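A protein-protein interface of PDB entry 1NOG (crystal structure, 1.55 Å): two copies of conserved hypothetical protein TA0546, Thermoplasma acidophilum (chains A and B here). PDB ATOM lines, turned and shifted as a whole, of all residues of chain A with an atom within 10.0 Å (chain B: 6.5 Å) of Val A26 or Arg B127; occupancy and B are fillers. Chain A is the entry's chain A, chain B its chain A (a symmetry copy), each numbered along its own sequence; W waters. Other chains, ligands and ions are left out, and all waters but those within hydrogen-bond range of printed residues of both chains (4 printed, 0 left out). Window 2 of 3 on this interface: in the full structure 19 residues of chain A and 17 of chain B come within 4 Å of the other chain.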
ATOM      1  N   SER A  23     -28.026   4.800 -27.113  1.00  0.00           N
ATOM      2  CA  SER A  23     -28.905   5.185 -28.252  1.00  0.00           C
ATOM      3  C   SER A  23     -28.619   4.326 -29.484  1.00  0.00           C
ATOM      4  O   SER A  23     -27.924   4.754 -30.406  1.00  0.00           O
ATOM      5  CB  SER A  23     -28.699   6.666 -28.592  1.00  0.00           C
ATOM      6  OG  SER A  23     -29.577   7.084 -29.621  1.00  0.00           O
ATOM      7  N   PRO A  24     -29.145   3.089 -29.509  1.00  0.00           N
ATOM      8  CA  PRO A  24     -29.970   2.502 -28.448  1.00  0.00           C
ATOM      9  C   PRO A  24     -29.112   2.006 -27.288  1.00  0.00           C
ATOM     10  O   PRO A  24     -29.542   2.016 -26.135  1.00  0.00           O
ATOM     11  CB  PRO A  24     -30.683   1.365 -29.166  1.00  0.00           C
ATOM     12  CG  PRO A  24     -29.636   0.891 -30.119  1.00  0.00           C
ATOM     13  CD  PRO A  24     -29.081   2.189 -30.674  1.00  0.00           C
ATOM     14  N   VAL A  25     -27.896   1.574 -27.607  1.00  0.00           N
ATOM     15  CA  VAL A  25     -26.969   1.073 -26.601  1.00  0.00           C
ATOM     16  C   VAL A  25     -25.819   2.047 -26.359  1.00  0.00           C
ATOM     17  O   VAL A  25     -24.940   1.784 -25.540  1.00  0.00           O
ATOM     18  CB  VAL A  25     -26.370  -0.290 -27.018  1.00  0.00           C
ATOM     19  CG1 VAL A  25     -27.477  -1.321 -27.167  1.00  0.00           C
ATOM     20  CG2 VAL A  25     -25.595  -0.143 -28.320  1.00  0.00           C
ATOM     21  N   VAL A  26     -25.823   3.165 -27.077  1.00  0.00           N
ATOM     22  CA  VAL A  26     -24.772   4.162 -26.916  1.00  0.00           C
ATOM     23  C   VAL A  26     -24.789   4.697 -25.487  1.00  0.00           C
ATOM     24  O   VAL A  26     -23.742   4.993 -24.911  1.00  0.00           O
ATOM     25  CB  VAL A  26     -24.953   5.337 -27.908  1.00  0.00           C
ATOM     26  CG1 VAL A  26     -23.885   6.395 -27.671  1.00  0.00           C
ATOM     27  CG2 VAL A  26     -24.864   4.822 -29.338  1.00  0.00           C
ATOM     28  N   GLU A  27     -25.985   4.810 -24.918  1.00  0.00           N
ATOM     29  CA  GLU A  27     -26.144   5.298 -23.554  1.00  0.00           C
ATOM     30  C   GLU A  27     -25.553   4.283 -22.582  1.00  0.00           C
ATOM     31  O   GLU A  27     -24.905   4.650 -21.602  1.00  0.00           O
ATOM     32  CB  GLU A  27     -27.628   5.515 -23.247  1.00  0.00           C
ATOM     33  CG  GLU A  27     -27.909   6.185 -21.918  1.00  0.00           C
ATOM     34  CD  GLU A  27     -27.201   7.518 -21.772  1.00  0.00           C
ATOM     35  OE1 GLU A  27     -27.129   8.271 -22.767  1.00  0.00           O
ATOM     36  OE2 GLU A  27     -26.728   7.818 -20.657  1.00  0.00           O
ATOM     37  N   VAL A  28     -25.785   3.002 -22.853  1.00  0.00           N
ATOM     38  CA  VAL A  28     -25.255   1.943 -22.003  1.00  0.00           C
ATOM     39  C   VAL A  28     -23.733   1.950 -22.093  1.00  0.00           C
ATOM     40  O   VAL A  28     -23.042   1.869 -21.077  1.00  0.00           O
ATOM     41  CB  VAL A  28     -25.787   0.555 -22.439  1.00  0.00           C
ATOM     42  CG1 VAL A  28     -25.121  -0.548 -21.620  1.00  0.00           C
ATOM     43  CG2 VAL A  28     -27.292   0.503 -22.254  1.00  0.00           C
ATOM     44  N   GLN A  29     -23.214   2.049 -23.313  1.00  0.00           N
ATOM     45  CA  GLN A  29     -21.771   2.073 -23.522  1.00  0.00           C
ATOM     46  C   GLN A  29     -21.141   3.245 -22.782  1.00  0.00           C
ATOM     47  O   GLN A  29     -20.103   3.103 -22.134  1.00  0.00           O
ATOM     48  CB  GLN A  29     -21.451   2.174 -25.016  1.00  0.00           C
ATOM     49  CG  GLN A  29     -21.900   0.964 -25.815  1.00  0.00           C
ATOM     50  CD  GLN A  29     -21.152  -0.300 -25.430  1.00  0.00           C
ATOM     51  OE1 GLN A  29     -21.595  -1.408 -25.730  1.00  0.00           O
ATOM     52  NE2 GLN A  29     -20.007  -0.139 -24.772  1.00  0.00           N
ATOM     53  N   GLY A  30     -21.775   4.409 -22.880  1.00  0.00           N
ATOM     54  CA  GLY A  30     -21.254   5.583 -22.207  1.00  0.00           C
ATOM     55  C   GLY A  30     -21.254   5.428 -20.700  1.00  0.00           C
ATOM     56  O   GLY A  30     -20.335   5.893 -20.023  1.00  0.00           O
ATOM     57  N   THR A  31     -22.284   4.778 -20.167  1.00  0.00           N
ATOM     58  CA  THR A  31     -22.385   4.581 -18.730  1.00  0.00           C
ATOM     59  C   THR A  31     -21.345   3.573 -18.258  1.00  0.00           C
ATOM     60  O   THR A  31     -20.819   3.693 -17.153  1.00  0.00           O
ATOM     61  CB  THR A  31     -23.793   4.105 -18.332  1.00  0.00           C
ATOM     62  OG1 THR A  31     -24.765   5.042 -18.822  1.00  0.00           O
ATOM     63  CG2 THR A  31     -23.915   4.008 -16.821  1.00  0.00           C
ATOM     64  N   ILE A  32     -21.052   2.578 -19.091  1.00  0.00           N
ATOM     65  CA  ILE A  32     -20.038   1.587 -18.738  1.00  0.00           C
ATOM     66  C   ILE A  32     -18.711   2.332 -18.627  1.00  0.00           C
ATOM     67  O   ILE A  32     -17.932   2.106 -17.702  1.00  0.00           O
ATOM     68  CB  ILE A  32     -19.912   0.493 -19.819  1.00  0.00           C
ATOM     69  CG1 ILE A  32     -21.184  -0.354 -19.851  1.00  0.00           C
ATOM     70  CG2 ILE A  32     -18.689  -0.378 -19.541  1.00  0.00           C
ATOM     71  CD1 ILE A  32     -21.224  -1.346 -20.997  1.00  0.00           C
ATOM     72  N   ASP A  33     -18.465   3.226 -19.578  1.00  0.00           N
ATOM     73  CA  ASP A  33     -17.242   4.017 -19.589  1.00  0.00           C
ATOM     74  C   ASP A  33     -17.122   4.864 -18.326  1.00  0.00           C
ATOM     75  O   ASP A  33     -16.064   4.916 -17.697  1.00  0.00           O
ATOM     76  CB  ASP A  33     -17.223   4.927 -20.816  1.00  0.00           C
ATOM     77  CG  ASP A  33     -16.145   5.983 -20.737  1.00  0.00           C
ATOM     78  OD1 ASP A  33     -14.952   5.618 -20.707  1.00  0.00           O
ATOM     79  OD2 ASP A  33     -16.497   7.179 -20.695  1.00  0.00           O
ATOM     80  N   GLU A  34     -18.211   5.534 -17.962  1.00  0.00           N
ATOM     81  CA  GLU A  34     -18.218   6.375 -16.773  1.00  0.00           C
ATOM     82  C   GLU A  34     -17.954   5.518 -15.547  1.00  0.00           C
ATOM     83  O   GLU A  34     -17.150   5.878 -14.691  1.00  0.00           O
ATOM     84  CB  GLU A  34     -19.560   7.098 -16.614  1.00  0.00           C
ATOM     85  CG  GLU A  34     -19.520   8.201 -15.566  1.00  0.00           C
ATOM     86  CD  GLU A  34     -20.828   8.948 -15.441  1.00  0.00           C
ATOM     87  OE1 GLU A  34     -21.567   9.021 -16.445  1.00  0.00           O
ATOM     88  OE2 GLU A  34     -21.108   9.479 -14.345  1.00  0.00           O
ATOM     89  N   LEU A  35     -18.636   4.379 -15.463  1.00  0.00           N
ATOM     90  CA  LEU A  35     -18.449   3.486 -14.331  1.00  0.00           C
ATOM     91  C   LEU A  35     -16.993   3.040 -14.234  1.00  0.00           C
ATOM     92  O   LEU A  35     -16.402   3.048 -13.153  1.00  0.00           O
ATOM     93  CB  LEU A  35     -19.357   2.261 -14.468  1.00  0.00           C
ATOM     94  CG  LEU A  35     -19.185   1.166 -13.412  1.00  0.00           C
ATOM     95  CD1 LEU A  35     -19.383   1.730 -12.012  1.00  0.00           C
ATOM     96  CD2 LEU A  35     -20.186   0.058 -13.688  1.00  0.00           C
ATOM     97  N   GLY A  66     -19.051  -4.222 -22.384  1.00  0.00           N
ATOM     98  CA  GLY A  66     -19.284  -3.270 -23.454  1.00  0.00           C
ATOM     99  C   GLY A  66     -19.327  -3.942 -24.814  1.00  0.00           C
ATOM    100  O   GLY A  66     -20.171  -3.610 -25.646  1.00  0.00           O
ATOM    101  N   VAL A  69     -22.601  -5.971 -25.253  1.00  0.00           N
ATOM    102  CA  VAL A  69     -23.692  -5.062 -25.585  1.00  0.00           C
ATOM    103  C   VAL A  69     -23.601  -4.492 -27.002  1.00  0.00           C
ATOM    104  O   VAL A  69     -24.592  -4.478 -27.732  1.00  0.00           O
ATOM    105  CB  VAL A  69     -23.752  -3.885 -24.584  1.00  0.00           C
ATOM    106  CG1 VAL A  69     -24.825  -2.890 -25.008  1.00  0.00           C
ATOM    107  CG2 VAL A  69     -24.043  -4.412 -23.182  1.00  0.00           C
ATOM    108  N   SER A  70     -22.415  -4.027 -27.386  1.00  0.00           N
ATOM    109  CA  SER A  70     -22.207  -3.439 -28.709  1.00  0.00           C
ATOM    110  C   SER A  70     -22.319  -4.409 -29.882  1.00  0.00           C
ATOM    111  O   SER A  70     -22.911  -4.077 -30.910  1.00  0.00           O
ATOM    112  CB  SER A  70     -20.845  -2.743 -28.770  1.00  0.00           C
ATOM    113  OG  SER A  70     -20.832  -1.580 -27.962  1.00  0.00           O
ATOM    114  N   VAL A 121     -23.131   4.741  -9.718  1.00  0.00           N
ATOM    115  CA  VAL A 121     -23.038   4.727 -11.170  1.00  0.00           C
ATOM    116  C   VAL A 121     -23.359   3.327 -11.703  1.00  0.00           C
ATOM    117  O   VAL A 121     -23.936   3.184 -12.778  1.00  0.00           O
ATOM    118  CB  VAL A 121     -21.638   5.175 -11.648  1.00  0.00           C
ATOM    119  CG1 VAL A 121     -21.572   5.160 -13.170  1.00  0.00           C
ATOM    120  CG2 VAL A 121     -21.340   6.575 -11.122  1.00  0.00           C
ATOM    121  N   ARG A 124     -26.927   3.014 -11.898  1.00  0.00           N
ATOM    122  CA  ARG A 124     -27.427   3.782 -13.030  1.00  0.00           C
ATOM    123  C   ARG A 124     -27.241   2.909 -14.275  1.00  0.00           C
ATOM    124  O   ARG A 124     -28.096   2.880 -15.159  1.00  0.00           O
ATOM    125  CB  ARG A 124     -26.644   5.088 -13.197  1.00  0.00           C
ATOM    126  CG  ARG A 124     -27.210   5.994 -14.284  1.00  0.00           C
ATOM    127  CD  ARG A 124     -26.167   6.961 -14.792  1.00  0.00           C
ATOM    128  NE  ARG A 124     -25.571   7.753 -13.721  1.00  0.00           N
ATOM    129  CZ  ARG A 124     -24.458   8.464 -13.871  1.00  0.00           C
ATOM    130  NH1 ARG A 124     -23.837   8.475 -15.044  1.00  0.00           N
ATOM    131  NH2 ARG A 124     -23.962   9.151 -12.857  1.00  0.00           N
ATOM    132  N   LEU A 125     -26.119   2.197 -14.340  1.00  0.00           N
ATOM    133  CA  LEU A 125     -25.854   1.312 -15.473  1.00  0.00           C
ATOM    134  C   LEU A 125     -26.967   0.272 -15.568  1.00  0.00           C
ATOM    135  O   LEU A 125     -27.453  -0.028 -16.658  1.00  0.00           O
ATOM    136  CB  LEU A 125     -24.497   0.616 -15.310  1.00  0.00           C
ATOM    137  CG  LEU A 125     -24.165  -0.464 -16.349  1.00  0.00           C
ATOM    138  CD1 LEU A 125     -24.216   0.114 -17.761  1.00  0.00           C
ATOM    139  CD2 LEU A 125     -22.785  -1.033 -16.060  1.00  0.00           C
ATOM    140  N   ARG A 128     -29.964   1.810 -17.119  1.00  0.00           N
ATOM    141  CA  ARG A 128     -29.774   2.042 -18.547  1.00  0.00           C
ATOM    142  C   ARG A 128     -29.875   0.740 -19.339  1.00  0.00           C
ATOM    143  O   ARG A 128     -30.385   0.724 -20.462  1.00  0.00           O
ATOM    144  CB  ARG A 128     -28.419   2.710 -18.799  1.00  0.00           C
ATOM    145  CG  ARG A 128     -28.288   4.093 -18.167  1.00  0.00           C
ATOM    146  CD  ARG A 128     -29.241   5.102 -18.798  1.00  0.00           C
ATOM    147  NE  ARG A 128     -29.011   6.444 -18.268  1.00  0.00           N
ATOM    148  CZ  ARG A 128     -29.553   6.920 -17.152  1.00  0.00           C
ATOM    149  NH1 ARG A 128     -30.381   6.175 -16.433  1.00  0.00           N
ATOM    150  NH2 ARG A 128     -29.244   8.141 -16.738  1.00  0.00           N
ATOM    151  N   ILE A 129     -29.394  -0.352 -18.757  1.00  0.00           N
ATOM    152  CA  ILE A 129     -29.459  -1.646 -19.428  1.00  0.00           C
ATOM    153  C   ILE A 129     -30.916  -2.076 -19.547  1.00  0.00           C
ATOM    154  O   ILE A 129     -31.350  -2.548 -20.599  1.00  0.00           O
ATOM    155  CB  ILE A 129     -28.668  -2.725 -18.654  1.00  0.00           C
ATOM    156  CG1 ILE A 129     -27.172  -2.408 -18.719  1.00  0.00           C
ATOM    157  CG2 ILE A 129     -28.950  -4.109 -19.246  1.00  0.00           C
ATOM    158  CD1 ILE A 129     -26.315  -3.293 -17.831  1.00  0.00           C
ATOM    159  N   ALA A 131     -33.562  -0.177 -19.620  1.00  0.00           N
ATOM    160  CA  ALA A 131     -34.215   0.677 -20.609  1.00  0.00           C
ATOM    161  C   ALA A 131     -33.863   0.275 -22.039  1.00  0.00           C
ATOM    162  O   ALA A 131     -34.734   0.213 -22.907  1.00  0.00           O
ATOM    163  CB  ALA A 131     -33.836   2.133 -20.373  1.00  0.00           C
ATOM    164  N   ALA A 132     -32.585  -0.002 -22.281  1.00  0.00           N
ATOM    165  CA  ALA A 132     -32.128  -0.384 -23.612  1.00  0.00           C
ATOM    166  C   ALA A 132     -32.618  -1.763 -24.038  1.00  0.00           C
ATOM    167  O   ALA A 132     -32.858  -2.004 -25.221  1.00  0.00           O
ATOM    168  CB  ALA A 132     -30.604  -0.337 -23.672  1.00  0.00           C
ATOM    169  N   SER A 133     -32.770  -2.665 -23.072  1.00  0.00           N
ATOM    170  CA  SER A 133     -33.209  -4.027 -23.357  1.00  0.00           C
ATOM    171  C   SER A 133     -34.616  -4.087 -23.943  1.00  0.00           C
ATOM    172  O   SER A 133     -34.981  -5.067 -24.590  1.00  0.00           O
ATOM    173  CB  SER A 133     -33.154  -4.880 -22.087  1.00  0.00           C
ATOM    174  OG  SER A 133     -34.129  -4.459 -21.150  1.00  0.00           O
ATOM    175  N   LEU A 135     -35.662  -2.085 -26.179  1.00  0.00           N
ATOM    176  CA  LEU A 135     -35.564  -1.625 -27.560  1.00  0.00           C
ATOM    177  C   LEU A 135     -34.593  -2.456 -28.393  1.00  0.00           C
ATOM    178  O   LEU A 135     -34.703  -2.505 -29.619  1.00  0.00           O
ATOM    179  CB  LEU A 135     -35.133  -0.155 -27.585  1.00  0.00           C
ATOM    180  CG  LEU A 135     -36.034   0.829 -26.833  1.00  0.00           C
ATOM    181  CD1 LEU A 135     -35.407   2.213 -26.849  1.00  0.00           C
ATOM    182  CD2 LEU A 135     -37.416   0.856 -27.472  1.00  0.00           C
ATOM    183  N   THR A 136     -33.645  -3.107 -27.727  1.00  0.00           N
ATOM    184  CA  THR A 136     -32.656  -3.926 -28.415  1.00  0.00           C
ATOM    185  C   THR A 136     -32.329  -5.183 -27.613  1.00  0.00           C
ATOM    186  O   THR A 136     -32.488  -5.213 -26.393  1.00  0.00           O
ATOM    187  CB  THR A 136     -31.355  -3.130 -28.659  1.00  0.00           C
ATOM    188  OG1 THR A 136     -30.425  -3.938 -29.391  1.00  0.00           O
ATOM    189  CG2 THR A 136     -30.727  -2.714 -27.339  1.00  0.00           C
ATOM    190  N   ILE A 138     -30.253  -7.741 -25.619  1.00  0.00           N
ATOM    191  CA  ILE A 138     -29.070  -7.716 -24.768  1.00  0.00           C
ATOM    192  C   ILE A 138     -29.031  -8.995 -23.944  1.00  0.00           C
ATOM    193  O   ILE A 138     -30.024  -9.373 -23.323  1.00  0.00           O
ATOM    194  CB  ILE A 138     -29.086  -6.498 -23.815  1.00  0.00           C
ATOM    195  CG1 ILE A 138     -29.070  -5.201 -24.629  1.00  0.00           C
ATOM    196  CG2 ILE A 138     -27.883  -6.551 -22.880  1.00  0.00           C
ATOM    197  CD1 ILE A 138     -29.166  -3.945 -23.791  1.00  0.00           C
ATOM    198  N   ALA B 120     -15.494  11.097 -19.130  1.00  0.00           N
ATOM    199  CA  ALA B 120     -16.750  10.360 -19.247  1.00  0.00           C
ATOM    200  C   ALA B 120     -17.936  11.320 -19.233  1.00  0.00           C
ATOM    201  O   ALA B 120     -18.909  11.126 -19.958  1.00  0.00           O
ATOM    202  CB  ALA B 120     -16.875   9.343 -18.119  1.00  0.00           C
ATOM    203  N   SER B 122     -17.821  14.404 -20.238  1.00  0.00           N
ATOM    204  CA  SER B 122     -17.779  15.164 -21.482  1.00  0.00           C
ATOM    205  C   SER B 122     -18.426  14.346 -22.599  1.00  0.00           C
ATOM    206  O   SER B 122     -19.090  14.894 -23.476  1.00  0.00           O
ATOM    207  CB  SER B 122     -16.337  15.515 -21.857  1.00  0.00           C
ATOM    208  OG  SER B 122     -15.653  14.389 -22.375  1.00  0.00           O
ATOM    209  N   ARG B 123     -18.232  13.031 -22.564  1.00  0.00           N
ATOM    210  CA  ARG B 123     -18.824  12.163 -23.580  1.00  0.00           C
ATOM    211  C   ARG B 123     -20.338  12.122 -23.365  1.00  0.00           C
ATOM    212  O   ARG B 123     -21.111  12.013 -24.321  1.00  0.00           O
ATOM    213  CB  ARG B 123     -18.210  10.758 -23.519  1.00  0.00           C
ATOM    214  CG  ARG B 123     -16.794  10.713 -24.099  1.00  0.00           C
ATOM    215  CD  ARG B 123     -16.153   9.334 -23.990  1.00  0.00           C
ATOM    216  NE  ARG B 123     -16.817   8.329 -24.820  1.00  0.00           N
ATOM    217  CZ  ARG B 123     -16.786   8.306 -26.149  1.00  0.00           C
ATOM    218  NH1 ARG B 123     -16.124   9.237 -26.822  1.00  0.00           N
ATOM    219  NH2 ARG B 123     -17.418   7.342 -26.809  1.00  0.00           N
ATOM    220  N   ARG B 124     -20.766  12.222 -22.109  1.00  0.00           N
ATOM    221  CA  ARG B 124     -22.191  12.244 -21.812  1.00  0.00           C
ATOM    222  C   ARG B 124     -22.741  13.557 -22.378  1.00  0.00           C
ATOM    223  O   ARG B 124     -23.841  13.595 -22.928  1.00  0.00           O
ATOM    224  CB  ARG B 124     -22.439  12.194 -20.302  1.00  0.00           C
ATOM    225  CG  ARG B 124     -23.915  12.081 -19.937  1.00  0.00           C
ATOM    226  CD  ARG B 124     -24.173  12.566 -18.530  1.00  0.00           C
ATOM    227  NE  ARG B 124     -23.345  11.882 -17.542  1.00  0.00           N
ATOM    228  CZ  ARG B 124     -23.190  12.312 -16.295  1.00  0.00           C
ATOM    229  NH1 ARG B 124     -23.809  13.417 -15.898  1.00  0.00           N
ATOM    230  NH2 ARG B 124     -22.415  11.653 -15.451  1.00  0.00           N
ATOM    231  N   LEU B 125     -21.970  14.633 -22.243  1.00  0.00           N
ATOM    232  CA  LEU B 125     -22.390  15.930 -22.770  1.00  0.00           C
ATOM    233  C   LEU B 125     -22.610  15.811 -24.276  1.00  0.00           C
ATOM    234  O   LEU B 125     -23.587  16.336 -24.810  1.00  0.00           O
ATOM    235  CB  LEU B 125     -21.331  17.001 -22.477  1.00  0.00           C
ATOM    236  CG  LEU B 125     -21.569  18.376 -23.117  1.00  0.00           C
ATOM    237  CD1 LEU B 125     -22.922  18.940 -22.690  1.00  0.00           C
ATOM    238  CD2 LEU B 125     -20.449  19.321 -22.710  1.00  0.00           C
ATOM    239  N   GLU B 126     -21.707  15.115 -24.959  1.00  0.00           N
ATOM    240  CA  GLU B 126     -21.838  14.928 -26.402  1.00  0.00           C
ATOM    241  C   GLU B 126     -23.163  14.248 -26.712  1.00  0.00           C
ATOM    242  O   GLU B 126     -23.887  14.668 -27.614  1.00  0.00           O
ATOM    243  CB  GLU B 126     -20.700  14.064 -26.948  1.00  0.00           C
ATOM    244  CG  GLU B 126     -19.337  14.728 -26.942  1.00  0.00           C
ATOM    245  CD  GLU B 126     -18.277  13.850 -27.581  1.00  0.00           C
ATOM    246  OE1 GLU B 126     -18.402  13.549 -28.787  1.00  0.00           O
ATOM    247  OE2 GLU B 126     -17.322  13.456 -26.880  1.00  0.00           O
ATOM    248  N   ARG B 127     -23.477  13.196 -25.962  1.00  0.00           N
ATOM    249  CA  ARG B 127     -24.720  12.464 -26.178  1.00  0.00           C
ATOM    250  C   ARG B 127     -25.935  13.353 -25.952  1.00  0.00           C
ATOM    251  O   ARG B 127     -26.908  13.286 -26.706  1.00  0.00           O
ATOM    252  CB  ARG B 127     -24.798  11.239 -25.256  1.00  0.00           C
ATOM    253  CG  ARG B 127     -23.726  10.193 -25.510  1.00  0.00           C
ATOM    254  CD  ARG B 127     -24.101   8.854 -24.883  1.00  0.00           C
ATOM    255  NE  ARG B 127     -24.262   8.913 -23.431  1.00  0.00           N
ATOM    256  CZ  ARG B 127     -23.257   8.938 -22.559  1.00  0.00           C
ATOM    257  NH1 ARG B 127     -21.998   8.912 -22.979  1.00  0.00           N
ATOM    258  NH2 ARG B 127     -23.513   8.976 -21.259  1.00  0.00           N
ATOM    259  N   ARG B 128     -25.882  14.187 -24.919  1.00  0.00           N
ATOM    260  CA  ARG B 128     -26.996  15.078 -24.615  1.00  0.00           C
ATOM    261  C   ARG B 128     -27.168  16.141 -25.698  1.00  0.00           C
ATOM    262  O   ARG B 128     -28.291  16.534 -26.023  1.00  0.00           O
ATOM    263  CB  ARG B 128     -26.786  15.741 -23.251  1.00  0.00           C
ATOM    264  CG  ARG B 128     -26.757  14.757 -22.086  1.00  0.00           C
ATOM    265  CD  ARG B 128     -28.104  14.073 -21.881  1.00  0.00           C
ATOM    266  NE  ARG B 128     -28.090  13.232 -20.687  1.00  0.00           N
ATOM    267  CZ  ARG B 128     -27.663  11.973 -20.652  1.00  0.00           C
ATOM    268  NH1 ARG B 128     -27.220  11.381 -21.751  1.00  0.00           N
ATOM    269  NH2 ARG B 128     -27.655  11.312 -19.503  1.00  0.00           N
ATOM    270  N   ILE B 129     -26.058  16.606 -26.260  1.00  0.00           N
ATOM    271  CA  ILE B 129     -26.120  17.613 -27.314  1.00  0.00           C
ATOM    272  C   ILE B 129     -26.761  17.001 -28.553  1.00  0.00           C
ATOM    273  O   ILE B 129     -27.618  17.618 -29.189  1.00  0.00           O
ATOM    274  CB  ILE B 129     -24.714  18.143 -27.673  1.00  0.00           C
ATOM    275  CG1 ILE B 129     -24.154  18.948 -26.499  1.00  0.00           C
ATOM    276  CG2 ILE B 129     -24.785  19.011 -28.933  1.00  0.00           C
ATOM    277  CD1 ILE B 129     -22.699  19.353 -26.666  1.00  0.00           C
ATOM    278  N   VAL B 130     -26.352  15.784 -28.894  1.00  0.00           N
ATOM    279  CA  VAL B 130     -26.911  15.106 -30.055  1.00  0.00           C
ATOM    280  C   VAL B 130     -28.419  14.932 -29.883  1.00  0.00           C
ATOM    281  O   VAL B 130     -29.190  15.202 -30.805  1.00  0.00           O
ATOM    282  CB  VAL B 130     -26.250  13.721 -30.268  1.00  0.00           C
ATOM    283  CG1 VAL B 130     -26.987  12.943 -31.352  1.00  0.00           C
ATOM    284  CG2 VAL B 130     -24.789  13.903 -30.661  1.00  0.00           C
ATOM    285  N   ALA B 131     -28.841  14.498 -28.700  1.00  0.00           N
ATOM    286  CA  ALA B 131     -30.263  14.296 -28.430  1.00  0.00           C
ATOM    287  C   ALA B 131     -31.057  15.596 -28.524  1.00  0.00           C
ATOM    288  O   ALA B 131     -32.140  15.631 -29.109  1.00  0.00           O
ATOM    289  CB  ALA B 131     -30.450  13.674 -27.054  1.00  0.00           C
ATOM    290  N   ALA B 132     -30.515  16.667 -27.950  1.00  0.00           N
ATOM    291  CA  ALA B 132     -31.188  17.961 -27.963  1.00  0.00           C
ATOM    292  C   ALA B 132     -31.233  18.595 -29.348  1.00  0.00           C
ATOM    293  O   ALA B 132     -32.185  19.300 -29.681  1.00  0.00           O
ATOM    294  CB  ALA B 132     -30.506  18.910 -26.982  1.00  0.00           C
ATOM    295  N   LEU B 143     -21.175  20.844 -30.578  1.00  0.00           N
ATOM    296  CA  LEU B 143     -20.877  19.419 -30.522  1.00  0.00           C
ATOM    297  C   LEU B 143     -19.413  19.174 -30.859  1.00  0.00           C
ATOM    298  O   LEU B 143     -18.760  18.332 -30.244  1.00  0.00           O
ATOM    299  CB  LEU B 143     -21.765  18.640 -31.496  1.00  0.00           C
ATOM    300  CG  LEU B 143     -21.505  17.130 -31.552  1.00  0.00           C
ATOM    301  CD1 LEU B 143     -21.695  16.515 -30.172  1.00  0.00           C
ATOM    302  CD2 LEU B 143     -22.449  16.487 -32.555  1.00  0.00           C
HETATM  303  O   HOH W   1     -20.037   8.822 -20.821  1.00  0.00           O
HETATM  304  O   HOH W   2     -26.146   8.601 -18.354  1.00  0.00           O
HETATM  305  O   HOH W   3     -22.168   8.273 -18.872  1.00  0.00           O
HETATM  306  O   HOH W   4     -18.215   7.474 -22.706  1.00  0.00           O
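Arg A124 touches its own counterpart, Arg B124. Positions printed for both chains: 124, 125, 128, 129, 131 and 132. Of the 9 pairs that touch across the chains among the printed residues, 1 has its exchanged pair printed and touching as well.
Water W2 bridges OE2 of Glu A27 and NH2 of Arg B128. Water W3 lies within hydrogen-bond range of the side-chain carboxylate (OE1) of Glu A34 (2.6 Å), the guanidinium group (NH2) of Arg B127 (2.8 Å) and the backbone carbonyl oxygen (O) of Gly A30 (3.2 Å). Water W4 lies within hydrogen-bond range of OD2 of Asp A33 (2.7 Å) and NE of Arg B123 (2.7 Å). Water W1 lies within hydrogen-bond range of O of Ala B120 (2.7 Å), NH1 of Arg B127 (2.9 Å) and O of Gly A30 (3.1 Å).
Printed residues of chain A that touch a printed residue of chain B: Val A26, Glu A27, Gly A30, Asp A33, Glu A34 and Arg A124. Hydrophobic or aromatic side chains of chain A that line the printed part of chain B: Val A26. Of the 13 printed residues of chain B, 5 touch a printed residue of chain A. Printed residues of chain B that touch a printed residue of chain A: Ala B120, Arg B123, Arg B124, Arg B127 and Arg B128. Hydrophobic or aromatic side chains of chain B within 4 Å of the printed part of chain A: Ala B120. Among the printed residues, 9 pairs touch across the chains. Among the printed residues, Asp or Glu carboxylates within 4 Å of a Lys or Arg side-chain nitrogen of the other chain: Glu A27 with Arg B127 (3.0 Å), Glu A27 with Arg B128 (3.3 Å) and Glu A34 with Arg B124 (2.8 Å).
Among the printed residues, merely in contact across the chains: Val A26 with Arg B127 (3.7 Å), Gly A30 with Arg B127 (3.5 Å), Asp A33 with Ala B120 (3.4 Å), Asp A33 with Arg B123 (3.95 Å), Glu A34 with Ala B120 (3.5 Å) and Arg A124 with Arg B124 (3.5 Å).
Of chain A, only Val A26 (3.7 Å), Glu A27 (3.0 Å) and Gly A30 (3.5 Å) come within 4 Å of Arg B127. No residue of chain A comes within 4 Å of Val B130. Of the printed residues of chain B, Asp A33 touches Ala B120 (3.4 Å) and Arg B123 (3.95 Å). Of the printed residues of chain A, Ala B120 touches Asp A33 and Glu A34. Of the printed residues of chain A, Arg B124 touches Glu A34 and Arg A124. Printed residues of chain B within 4 Å of Gly A30: Arg B127 (3.5 Å). Of the printed residues of chain B, Arg A124 touches Arg B124 (3.5 Å). Ser A23 touches none of the printed residues of chain B. The nearest printed residue of chain B that does not touch Val A26 is Arg B123 (6.6 Å). The nearest residue of chain A that does not touch Arg B127 is Thr A31 (4.5 Å).
The backbone carbonyl oxygen (O) of Glu A27 lies within hydrogen-bond range of the side-chain hydroxyl (OG1) of Thr A31, 2.8 Å away. The side-chain carboxylate (OE2) of Glu A27 is in salt-bridge range of the guanidinium group (NE) of Arg A128 (3.6 Å). The side-chain carboxylate (OE1) of Glu A34 is in salt-bridge range of the guanidinium group (NH1) of Arg A124 (2.7 Å). The backbone carbonyl oxygen (O) of Arg B123 sits close to the guanidinium group (NH1) of Arg B127 (3.5 Å).
OE1 of Glu A27 is in salt-bridge range of NE of Arg B127 (3.0 Å). OE1 of Glu A27 is in salt-bridge range of NH1 of Arg B128, at 3.3 Å. NH2 of Arg B124 lies within salt-bridge range of OE2 of Glu A34 (2.8 Å).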
